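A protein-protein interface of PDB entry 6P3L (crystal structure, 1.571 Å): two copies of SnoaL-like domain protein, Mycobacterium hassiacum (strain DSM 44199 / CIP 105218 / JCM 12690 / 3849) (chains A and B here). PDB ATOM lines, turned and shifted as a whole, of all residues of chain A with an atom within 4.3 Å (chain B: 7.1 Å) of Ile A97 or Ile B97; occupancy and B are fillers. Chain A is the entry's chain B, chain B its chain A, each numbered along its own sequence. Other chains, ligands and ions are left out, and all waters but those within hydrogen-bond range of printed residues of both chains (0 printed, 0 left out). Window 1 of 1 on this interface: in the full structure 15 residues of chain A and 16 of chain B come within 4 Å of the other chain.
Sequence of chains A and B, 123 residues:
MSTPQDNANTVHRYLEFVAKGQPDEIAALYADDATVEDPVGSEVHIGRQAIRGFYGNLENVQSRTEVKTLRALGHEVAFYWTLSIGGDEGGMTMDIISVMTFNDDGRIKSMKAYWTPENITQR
Arg A71 touches Ile B96, and with the chains exchanged Ile A96 touches Arg B71.
Arg A71 touches Tyr B114, and with the chains exchanged Tyr A114 touches Arg B71.
Tyr A80 touches Thr B69, but with the chains exchanged Thr A69 does not touch Tyr B80 (4.2 Å).
Ile A97 touches its own counterpart, Ile B97.
10 positions are printed for both chains.
Of the 14 pairs that touch across the chains among the printed residues, 8 have their exchanged pair printed and touching as well.
Printed residues of chain B within 4 Å of Ile A97: Arg B71 and Ile B97.
Ile B97 touches just these residues of chain A: Arg A71 (3.6 Å) and Ile A97 (3.97 Å).
Of the printed residues of chain A, Ala B78 touches Tyr A114.
Of the printed residues of chain A, Val B99 touches Tyr A114.
Of the printed residues of chain A, Asn B119 touches Arg A71 (3.3 Å).
Of the printed residues of chain A, Trp B115 touches Arg A71.
The nearest residue of chain B that does not touch Ile A97 is Thr B69 (4.1 Å).
The nearest residue of chain A that does not touch Ile B97 is Thr A69 (4.1 Å).
OG1 of Thr B69 sits at hydrogen-bond distance from NE of Arg B71, at 2.9 Å.
N of Tyr B80 sits at hydrogen-bond distance from O of Thr B69 (2.9 Å).
The side-chain carboxylate (OD2) of Asp B95 lies within hydrogen-bond range of the side-chain hydroxyl (OH) of Tyr B80.
O of Trp B81 sits at hydrogen-bond distance from N of Ile B96, at 2.8 Å.
The backbone NH (N) of Lys B112 lies within hydrogen-bond range of the backbone carbonyl oxygen (O) of Val B99.
N of Tyr A114 sits at hydrogen-bond distance from O of Ile A97 (2.7 Å).
Among the printed residues, merely in contact across the chains: Arg A71 with Ile B96 (3.7 Å), Arg A71 with Ile B97 (3.6 Å), Arg A71 with Trp B115 (3.9 Å), Tyr A80 with Thr B69 (3.9 Å), Tyr A80 with Tyr B80 (3.7 Å), Ile A96 with Arg B71 (3.8 Å), Ile A97 with Arg B71 (3.7 Å), Ile A97 with Ile B97 (3.97 Å), Tyr A114 with Ala B78 (3.4 Å) and Tyr A114 with Val B99 (3.6 Å).
NH1 of Arg B71 sits at hydrogen-bond distance from O of Tyr A114, 2.9 Å away.
The side-chain carboxylate of Asp B95 is in salt-bridge range of the guanidinium group of Arg A71.
The guanidinium group (NH1) of Arg A71 lies within hydrogen-bond range of the backbone carbonyl oxygen (O) of Tyr B114 (2.9 Å).
NH2 of Arg A71 sits close to ND2 of Asn B119, at 3.3 Å.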
ATOM      1  N   THR A  69     -17.634   1.116  17.463  1.00  0.00           N
ATOM      2  CA  THR A  69     -17.586  -0.091  16.653  1.00  0.00           C
ATOM      3  C   THR A  69     -16.404  -0.936  17.106  1.00  0.00           C
ATOM      4  O   THR A  69     -15.374  -0.417  17.554  1.00  0.00           O
ATOM      5  CB  THR A  69     -17.485   0.231  15.152  1.00  0.00           C
ATOM      6  OG1 THR A  69     -17.485  -0.987  14.394  1.00  0.00           O
ATOM      7  CG2 THR A  69     -16.213   1.000  14.833  1.00  0.00           C
ATOM      8  N   ARG A  71     -14.249  -4.671  16.054  1.00  0.00           N
ATOM      9  CA  ARG A  71     -14.015  -5.762  15.111  1.00  0.00           C
ATOM     10  C   ARG A  71     -12.998  -6.716  15.721  1.00  0.00           C
ATOM     11  O   ARG A  71     -11.803  -6.393  15.811  1.00  0.00           O
ATOM     12  CB  ARG A  71     -13.529  -5.235  13.754  1.00  0.00           C
ATOM     13  CG  ARG A  71     -14.540  -4.300  13.034  1.00  0.00           C
ATOM     14  CD  ARG A  71     -14.226  -2.842  13.195  1.00  0.00           C
ATOM     15  NE  ARG A  71     -15.350  -1.974  12.842  1.00  0.00           N
ATOM     16  CZ  ARG A  71     -15.578  -1.458  11.634  1.00  0.00           C
ATOM     17  NH1 ARG A  71     -14.770  -1.702  10.617  1.00  0.00           N
ATOM     18  NH2 ARG A  71     -16.625  -0.678  11.448  1.00  0.00           N
ATOM     19  N   PHE A  79     -10.949  -1.375  17.967  1.00  0.00           N
ATOM     20  CA  PHE A  79     -12.179  -0.769  18.456  1.00  0.00           C
ATOM     21  C   PHE A  79     -12.049   0.740  18.527  1.00  0.00           C
ATOM     22  O   PHE A  79     -10.993   1.282  18.868  1.00  0.00           O
ATOM     23  CB  PHE A  79     -12.633  -1.353  19.813  1.00  0.00           C
ATOM     24  CG  PHE A  79     -11.595  -1.369  20.906  1.00  0.00           C
ATOM     25  CD1 PHE A  79     -11.727  -0.539  22.000  1.00  0.00           C
ATOM     26  CD2 PHE A  79     -10.539  -2.253  20.880  1.00  0.00           C
ATOM     27  CE1 PHE A  79     -10.815  -0.568  23.034  1.00  0.00           C
ATOM     28  CE2 PHE A  79      -9.621  -2.293  21.916  1.00  0.00           C
ATOM     29  CZ  PHE A  79      -9.757  -1.435  22.987  1.00  0.00           C
ATOM     30  N   TYR A  80     -13.137   1.400  18.130  1.00  0.00           N
ATOM     31  CA  TYR A  80     -13.273   2.849  18.107  1.00  0.00           C
ATOM     32  C   TYR A  80     -14.249   3.197  19.219  1.00  0.00           C
ATOM     33  O   TYR A  80     -15.369   2.671  19.244  1.00  0.00           O
ATOM     34  CB  TYR A  80     -13.777   3.285  16.732  1.00  0.00           C
ATOM     35  CG  TYR A  80     -13.933   4.765  16.495  1.00  0.00           C
ATOM     36  CD1 TYR A  80     -13.048   5.684  17.035  1.00  0.00           C
ATOM     37  CD2 TYR A  80     -14.954   5.235  15.683  1.00  0.00           C
ATOM     38  CE1 TYR A  80     -13.195   7.036  16.785  1.00  0.00           C
ATOM     39  CE2 TYR A  80     -15.107   6.575  15.426  1.00  0.00           C
ATOM     40  CZ  TYR A  80     -14.234   7.473  15.980  1.00  0.00           C
ATOM     41  OH  TYR A  80     -14.405   8.815  15.708  1.00  0.00           O
ATOM     42  N   ILE A  96     -11.171   7.472  20.589  1.00  0.00           N
ATOM     43  CA  ILE A  96      -9.896   6.773  20.502  1.00  0.00           C
ATOM     44  C   ILE A  96     -10.054   5.575  19.582  1.00  0.00           C
ATOM     45  O   ILE A  96     -11.051   4.851  19.660  1.00  0.00           O
ATOM     46  CB  ILE A  96      -9.433   6.298  21.899  1.00  0.00           C
ATOM     47  CG1 ILE A  96      -9.355   7.470  22.884  1.00  0.00           C
ATOM     48  CG2 ILE A  96      -8.091   5.559  21.803  1.00  0.00           C
ATOM     49  CD1 ILE A  96      -9.314   7.031  24.333  1.00  0.00           C
ATOM     50  N   ILE A  97      -9.052   5.338  18.737  1.00  0.00           N
ATOM     51  CA  ILE A  97      -8.956   4.087  17.983  1.00  0.00           C
ATOM     52  C   ILE A  97      -7.898   3.250  18.674  1.00  0.00           C
ATOM     53  O   ILE A  97      -6.758   3.699  18.819  1.00  0.00           O
ATOM     54  CB  ILE A  97      -8.580   4.308  16.509  1.00  0.00           C
ATOM     55  CG1 ILE A  97      -9.667   5.098  15.792  1.00  0.00           C
ATOM     56  CG2 ILE A  97      -8.383   2.950  15.827  1.00  0.00           C
ATOM     57  CD1 ILE A  97      -9.307   5.503  14.367  1.00  0.00           C
ATOM     58  N   SER A  98      -8.260   2.027  19.074  1.00  0.00           N
ATOM     59  CA  SER A  98      -7.360   1.144  19.796  1.00  0.00           C
ATOM     60  C   SER A  98      -7.281  -0.197  19.083  1.00  0.00           C
ATOM     61  O   SER A  98      -8.240  -0.642  18.445  1.00  0.00           O
ATOM     62  CB  SER A  98      -7.823   0.919  21.245  1.00  0.00           C
ATOM     63  OG  SER A  98      -7.871   2.144  21.957  1.00  0.00           O
ATOM     64  N   LYS A 112      -2.239  -0.793  21.516  1.00  0.00           N
ATOM     65  CA  LYS A 112      -1.813   0.439  20.870  1.00  0.00           C
ATOM     66  C   LYS A 112      -3.015   1.363  20.812  1.00  0.00           C
ATOM     67  O   LYS A 112      -4.110   0.926  20.458  1.00  0.00           O
ATOM     68  CB  LYS A 112      -1.272   0.196  19.463  1.00  0.00           C
ATOM     69  CG  LYS A 112       0.115  -0.446  19.415  1.00  0.00           C
ATOM     70  CD  LYS A 112       0.626  -0.565  17.976  1.00  0.00           C
ATOM     71  CE  LYS A 112       2.080  -1.014  17.948  1.00  0.00           C
ATOM     72  NZ  LYS A 112       2.592  -1.222  16.567  1.00  0.00           N
ATOM     73  N   ALA A 113      -2.811   2.633  21.144  1.00  0.00           N
ATOM     74  CA  ALA A 113      -3.890   3.609  21.184  1.00  0.00           C
ATOM     75  C   ALA A 113      -3.553   4.768  20.256  1.00  0.00           C
ATOM     76  O   ALA A 113      -2.465   5.353  20.350  1.00  0.00           O
ATOM     77  CB  ALA A 113      -4.132   4.130  22.612  1.00  0.00           C
ATOM     78  N   TYR A 114      -4.478   5.090  19.361  1.00  0.00           N
ATOM     79  CA  TYR A 114      -4.281   6.129  18.348  1.00  0.00           C
ATOM     80  C   TYR A 114      -5.227   7.288  18.653  1.00  0.00           C
ATOM     81  O   TYR A 114      -6.427   7.217  18.369  1.00  0.00           O
ATOM     82  CB  TYR A 114      -4.525   5.580  16.943  1.00  0.00           C
ATOM     83  CG  TYR A 114      -3.680   4.375  16.562  1.00  0.00           C
ATOM     84  CD1 TYR A 114      -2.557   4.517  15.756  1.00  0.00           C
ATOM     85  CD2 TYR A 114      -4.013   3.105  17.002  1.00  0.00           C
ATOM     86  CE1 TYR A 114      -1.786   3.425  15.397  1.00  0.00           C
ATOM     87  CE2 TYR A 114      -3.252   1.998  16.654  1.00  0.00           C
ATOM     88  CZ  TYR A 114      -2.146   2.159  15.850  1.00  0.00           C
ATOM     89  OH  TYR A 114      -1.402   1.062  15.521  1.00  0.00           O
ATOM     90  N   VAL B  40      -7.779  -8.494   8.616  1.00  0.00           N
ATOM     91  CA  VAL B  40      -7.005  -9.102   9.683  1.00  0.00           C
ATOM     92  C   VAL B  40      -7.570 -10.480   9.988  1.00  0.00           C
ATOM     93  O   VAL B  40      -8.793 -10.699   9.999  1.00  0.00           O
ATOM     94  CB  VAL B  40      -6.986  -8.167  10.905  1.00  0.00           C
ATOM     95  CG1 VAL B  40      -6.438  -8.856  12.147  1.00  0.00           C
ATOM     96  CG2 VAL B  40      -6.141  -6.966  10.568  1.00  0.00           C
ATOM     97  N   THR B  69     -11.893   9.766  10.257  1.00  0.00           N
ATOM     98  CA  THR B  69     -10.893  10.296  11.170  1.00  0.00           C
ATOM     99  C   THR B  69      -9.572   9.592  10.891  1.00  0.00           C
ATOM    100  O   THR B  69      -9.555   8.414  10.523  1.00  0.00           O
ATOM    101  CB  THR B  69     -11.332  10.134  12.637  1.00  0.00           C
ATOM    102  OG1 THR B  69     -10.358  10.715  13.509  1.00  0.00           O
ATOM    103  CG2 THR B  69     -11.548   8.672  13.015  1.00  0.00           C
ATOM    104  N   LEU B  70      -8.481  10.335  11.023  1.00  0.00           N
ATOM    105  CA  LEU B  70      -7.152   9.844  10.683  1.00  0.00           C
ATOM    106  C   LEU B  70      -6.177  10.332  11.736  1.00  0.00           C
ATOM    107  O   LEU B  70      -6.121  11.535  12.017  1.00  0.00           O
ATOM    108  CB  LEU B  70      -6.733  10.336   9.296  1.00  0.00           C
ATOM    109  CG  LEU B  70      -5.397   9.844   8.738  1.00  0.00           C
ATOM    110  CD1 LEU B  70      -5.492   9.831   7.233  1.00  0.00           C
ATOM    111  CD2 LEU B  70      -4.211  10.696   9.169  1.00  0.00           C
ATOM    112  N   ARG B  71      -5.402   9.407  12.296  1.00  0.00           N
ATOM    113  CA  ARG B  71      -4.417   9.731  13.325  1.00  0.00           C
ATOM    114  C   ARG B  71      -3.043   9.250  12.874  1.00  0.00           C
ATOM    115  O   ARG B  71      -2.770   8.045  12.852  1.00  0.00           O
ATOM    116  CB  ARG B  71      -4.800   9.108  14.666  1.00  0.00           C
ATOM    117  CG  ARG B  71      -6.118   9.638  15.238  1.00  0.00           C
ATOM    118  CD  ARG B  71      -7.219   8.630  15.105  1.00  0.00           C
ATOM    119  NE  ARG B  71      -8.541   9.230  15.290  1.00  0.00           N
ATOM    120  CZ  ARG B  71      -9.203   9.311  16.439  1.00  0.00           C
ATOM    121  NH1 ARG B  71      -8.701   8.810  17.566  1.00  0.00           N
ATOM    122  NH2 ARG B  71     -10.390   9.893  16.448  1.00  0.00           N
ATOM    123  N   ALA B  78      -3.464   5.363  11.759  1.00  0.00           N
ATOM    124  CA  ALA B  78      -4.733   4.676  11.926  1.00  0.00           C
ATOM    125  C   ALA B  78      -5.814   5.550  11.325  1.00  0.00           C
ATOM    126  O   ALA B  78      -5.860   6.756  11.594  1.00  0.00           O
ATOM    127  CB  ALA B  78      -5.047   4.395  13.396  1.00  0.00           C
ATOM    128  N   PHE B  79      -6.682   4.949  10.514  1.00  0.00           N
ATOM    129  CA  PHE B  79      -7.731   5.732   9.886  1.00  0.00           C
ATOM    130  C   PHE B  79      -9.010   4.929   9.765  1.00  0.00           C
ATOM    131  O   PHE B  79      -8.994   3.731   9.478  1.00  0.00           O
ATOM    132  CB  PHE B  79      -7.303   6.300   8.513  1.00  0.00           C
ATOM    133  CG  PHE B  79      -6.717   5.301   7.531  1.00  0.00           C
ATOM    134  CD1 PHE B  79      -7.405   4.987   6.369  1.00  0.00           C
ATOM    135  CD2 PHE B  79      -5.448   4.763   7.707  1.00  0.00           C
ATOM    136  CE1 PHE B  79      -6.869   4.114   5.427  1.00  0.00           C
ATOM    137  CE2 PHE B  79      -4.904   3.899   6.771  1.00  0.00           C
ATOM    138  CZ  PHE B  79      -5.617   3.574   5.626  1.00  0.00           C
ATOM    139  N   TYR B  80     -10.107   5.616  10.050  1.00  0.00           N
ATOM    140  CA  TYR B  80     -11.457   5.091   9.962  1.00  0.00           C
ATOM    141  C   TYR B  80     -12.099   5.749   8.747  1.00  0.00           C
ATOM    142  O   TYR B  80     -12.137   6.984   8.658  1.00  0.00           O
ATOM    143  CB  TYR B  80     -12.206   5.401  11.263  1.00  0.00           C
ATOM    144  CG  TYR B  80     -13.623   4.880  11.371  1.00  0.00           C
ATOM    145  CD1 TYR B  80     -13.938   3.581  11.021  1.00  0.00           C
ATOM    146  CD2 TYR B  80     -14.638   5.690  11.858  1.00  0.00           C
ATOM    147  CE1 TYR B  80     -15.232   3.108  11.127  1.00  0.00           C
ATOM    148  CE2 TYR B  80     -15.931   5.226  11.974  1.00  0.00           C
ATOM    149  CZ  TYR B  80     -16.224   3.937  11.609  1.00  0.00           C
ATOM    150  OH  TYR B  80     -17.516   3.478  11.728  1.00  0.00           O
ATOM    151  N   TRP B  81     -12.563   4.937   7.798  1.00  0.00           N
ATOM    152  CA  TRP B  81     -12.957   5.468   6.504  1.00  0.00           C
ATOM    153  C   TRP B  81     -14.063   4.624   5.900  1.00  0.00           C
ATOM    154  O   TRP B  81     -14.307   3.490   6.316  1.00  0.00           O
ATOM    155  CB  TRP B  81     -11.783   5.514   5.536  1.00  0.00           C
ATOM    156  CG  TRP B  81     -11.127   4.207   5.279  1.00  0.00           C
ATOM    157  CD1 TRP B  81     -10.384   3.469   6.152  1.00  0.00           C
ATOM    158  CD2 TRP B  81     -11.125   3.489   4.042  1.00  0.00           C
ATOM    159  NE1 TRP B  81      -9.924   2.333   5.533  1.00  0.00           N
ATOM    160  CE2 TRP B  81     -10.370   2.316   4.241  1.00  0.00           C
ATOM    161  CE3 TRP B  81     -11.697   3.718   2.790  1.00  0.00           C
ATOM    162  CZ2 TRP B  81     -10.150   1.389   3.224  1.00  0.00           C
ATOM    163  CZ3 TRP B  81     -11.486   2.796   1.783  1.00  0.00           C
ATOM    164  CH2 TRP B  81     -10.721   1.644   2.005  1.00  0.00           C
ATOM    165  N   ASP B  95     -17.688   0.737   6.442  1.00  0.00           N
ATOM    166  CA  ASP B  95     -16.791   1.532   7.258  1.00  0.00           C
ATOM    167  C   ASP B  95     -15.696   0.625   7.791  1.00  0.00           C
ATOM    168  O   ASP B  95     -15.978  -0.434   8.359  1.00  0.00           O
ATOM    169  CB  ASP B  95     -17.545   2.214   8.402  1.00  0.00           C
ATOM    170  CG  ASP B  95     -18.374   1.246   9.225  1.00  0.00           C
ATOM    171  OD1 ASP B  95     -19.140   0.430   8.647  1.00  0.00           O
ATOM    172  OD2 ASP B  95     -18.267   1.312  10.466  1.00  0.00           O
ATOM    173  N   ILE B  96     -14.455   1.040   7.586  1.00  0.00           N
ATOM    174  CA  ILE B  96     -13.282   0.208   7.789  1.00  0.00           C
ATOM    175  C   ILE B  96     -12.350   0.919   8.755  1.00  0.00           C
ATOM    176  O   ILE B  96     -12.143   2.133   8.651  1.00  0.00           O
ATOM    177  CB  ILE B  96     -12.574  -0.054   6.445  1.00  0.00           C
ATOM    178  CG1 ILE B  96     -13.527  -0.750   5.467  1.00  0.00           C
ATOM    179  CG2 ILE B  96     -11.315  -0.860   6.636  1.00  0.00           C
ATOM    180  CD1 ILE B  96     -13.053  -0.736   4.035  1.00  0.00           C
ATOM    181  N   ILE B  97     -11.782   0.168   9.691  1.00  0.00           N
ATOM    182  CA  ILE B  97     -10.654   0.650  10.481  1.00  0.00           C
ATOM    183  C   ILE B  97      -9.395   0.057   9.883  1.00  0.00           C
ATOM    184  O   ILE B  97      -9.268  -1.167   9.798  1.00  0.00           O
ATOM    185  CB  ILE B  97     -10.765   0.266  11.964  1.00  0.00           C
ATOM    186  CG1 ILE B  97     -12.041   0.841  12.584  1.00  0.00           C
ATOM    187  CG2 ILE B  97      -9.519   0.775  12.707  1.00  0.00           C
ATOM    188  CD1 ILE B  97     -12.261   0.411  14.056  1.00  0.00           C
ATOM    189  N   SER B  98      -8.470   0.921   9.474  1.00  0.00           N
ATOM    190  CA  SER B  98      -7.213   0.500   8.882  1.00  0.00           C
ATOM    191  C   SER B  98      -6.030   1.057   9.659  1.00  0.00           C
ATOM    192  O   SER B  98      -6.089   2.160  10.206  1.00  0.00           O
ATOM    193  CB  SER B  98      -7.106   0.963   7.435  1.00  0.00           C
ATOM    194  OG  SER B  98      -8.075   0.323   6.627  1.00  0.00           O
ATOM    195  N   VAL B  99      -4.941   0.291   9.669  1.00  0.00           N
ATOM    196  CA  VAL B  99      -3.674   0.743  10.223  1.00  0.00           C
ATOM    197  C   VAL B  99      -2.587   0.481   9.202  1.00  0.00           C
ATOM    198  O   VAL B  99      -2.430  -0.657   8.740  1.00  0.00           O
ATOM    199  CB  VAL B  99      -3.334   0.045  11.553  1.00  0.00           C
ATOM    200  CG1 VAL B  99      -1.910   0.445  12.008  1.00  0.00           C
ATOM    201  CG2 VAL B  99      -4.366   0.418  12.601  1.00  0.00           C
ATOM    202  N   LYS B 112      -3.066  -3.248   7.663  1.00  0.00           N
ATOM    203  CA  LYS B 112      -4.032  -4.142   8.287  1.00  0.00           C
ATOM    204  C   LYS B 112      -5.403  -3.492   8.192  1.00  0.00           C
ATOM    205  O   LYS B 112      -5.544  -2.306   8.487  1.00  0.00           O
ATOM    206  CB  LYS B 112      -3.687  -4.424   9.753  1.00  0.00           C
ATOM    207  CG  LYS B 112      -2.549  -5.418   9.932  1.00  0.00           C
ATOM    208  CD  LYS B 112      -2.319  -5.765  11.386  1.00  0.00           C
ATOM    209  CE  LYS B 112      -1.254  -6.844  11.485  1.00  0.00           C
ATOM    210  NZ  LYS B 112      -0.894  -7.230  12.848  1.00  0.00           N
ATOM    211  N   ALA B 113      -6.405  -4.265   7.787  1.00  0.00           N
ATOM    212  CA  ALA B 113      -7.761  -3.760   7.598  1.00  0.00           C
ATOM    213  C   ALA B 113      -8.708  -4.557   8.484  1.00  0.00           C
ATOM    214  O   ALA B 113      -8.759  -5.793   8.398  1.00  0.00           O
ATOM    215  CB  ALA B 113      -8.167  -3.863   6.125  1.00  0.00           C
ATOM    216  N   TYR B 114      -9.451  -3.850   9.326  1.00  0.00           N
ATOM    217  CA  TYR B 114     -10.366  -4.431  10.299  1.00  0.00           C
ATOM    218  C   TYR B 114     -11.792  -4.124   9.847  1.00  0.00           C
ATOM    219  O   TYR B 114     -12.279  -3.008  10.025  1.00  0.00           O
ATOM    220  CB  TYR B 114     -10.088  -3.862  11.692  1.00  0.00           C
ATOM    221  CG  TYR B 114      -8.682  -4.088  12.208  1.00  0.00           C
ATOM    222  CD1 TYR B 114      -8.400  -5.127  13.089  1.00  0.00           C
ATOM    223  CD2 TYR B 114      -7.638  -3.234  11.845  1.00  0.00           C
ATOM    224  CE1 TYR B 114      -7.109  -5.327  13.577  1.00  0.00           C
ATOM    225  CE2 TYR B 114      -6.366  -3.415  12.324  1.00  0.00           C
ATOM    226  CZ  TYR B 114      -6.094  -4.456  13.187  1.00  0.00           C
ATOM    227  OH  TYR B 114      -4.799  -4.605  13.634  1.00  0.00           O
ATOM    228  N   TRP B 115     -12.460  -5.124   9.282  1.00  0.00           N
ATOM    229  CA  TRP B 115     -13.826  -4.999   8.788  1.00  0.00           C
ATOM    230  C   TRP B 115     -14.347  -6.409   8.576  1.00  0.00           C
ATOM    231  O   TRP B 115     -13.567  -7.352   8.410  1.00  0.00           O
ATOM    232  CB  TRP B 115     -13.895  -4.221   7.475  1.00  0.00           C
ATOM    233  CG  TRP B 115     -13.142  -4.899   6.382  1.00  0.00           C
ATOM    234  CD1 TRP B 115     -11.804  -4.810   6.139  1.00  0.00           C
ATOM    235  CD2 TRP B 115     -13.668  -5.804   5.390  1.00  0.00           C
ATOM    236  NE1 TRP B 115     -11.463  -5.594   5.057  1.00  0.00           N
ATOM    237  CE2 TRP B 115     -12.589  -6.212   4.583  1.00  0.00           C
ATOM    238  CE3 TRP B 115     -14.941  -6.313   5.113  1.00  0.00           C
ATOM    239  CZ2 TRP B 115     -12.749  -7.088   3.522  1.00  0.00           C
ATOM    240  CZ3 TRP B 115     -15.095  -7.179   4.068  1.00  0.00           C
ATOM    241  CH2 TRP B 115     -14.011  -7.557   3.281  1.00  0.00           C
ATOM    242  N   ASN B 119     -20.144  -4.887   8.655  1.00  0.00           N
ATOM    243  CA  ASN B 119     -19.930  -3.459   8.522  1.00  0.00           C
ATOM    244  C   ASN B 119     -20.446  -2.911   7.199  1.00  0.00           C
ATOM    245  O   ASN B 119     -20.246  -1.724   6.922  1.00  0.00           O
ATOM    246  CB  ASN B 119     -18.429  -3.162   8.679  1.00  0.00           C
ATOM    247  CG  ASN B 119     -17.860  -3.699   9.994  1.00  0.00           C
ATOM    248  OD1 ASN B 119     -16.849  -4.391  10.011  1.00  0.00           O
ATOM    249  ND2 ASN B 119     -18.529  -3.396  11.095  1.00  0.00           N
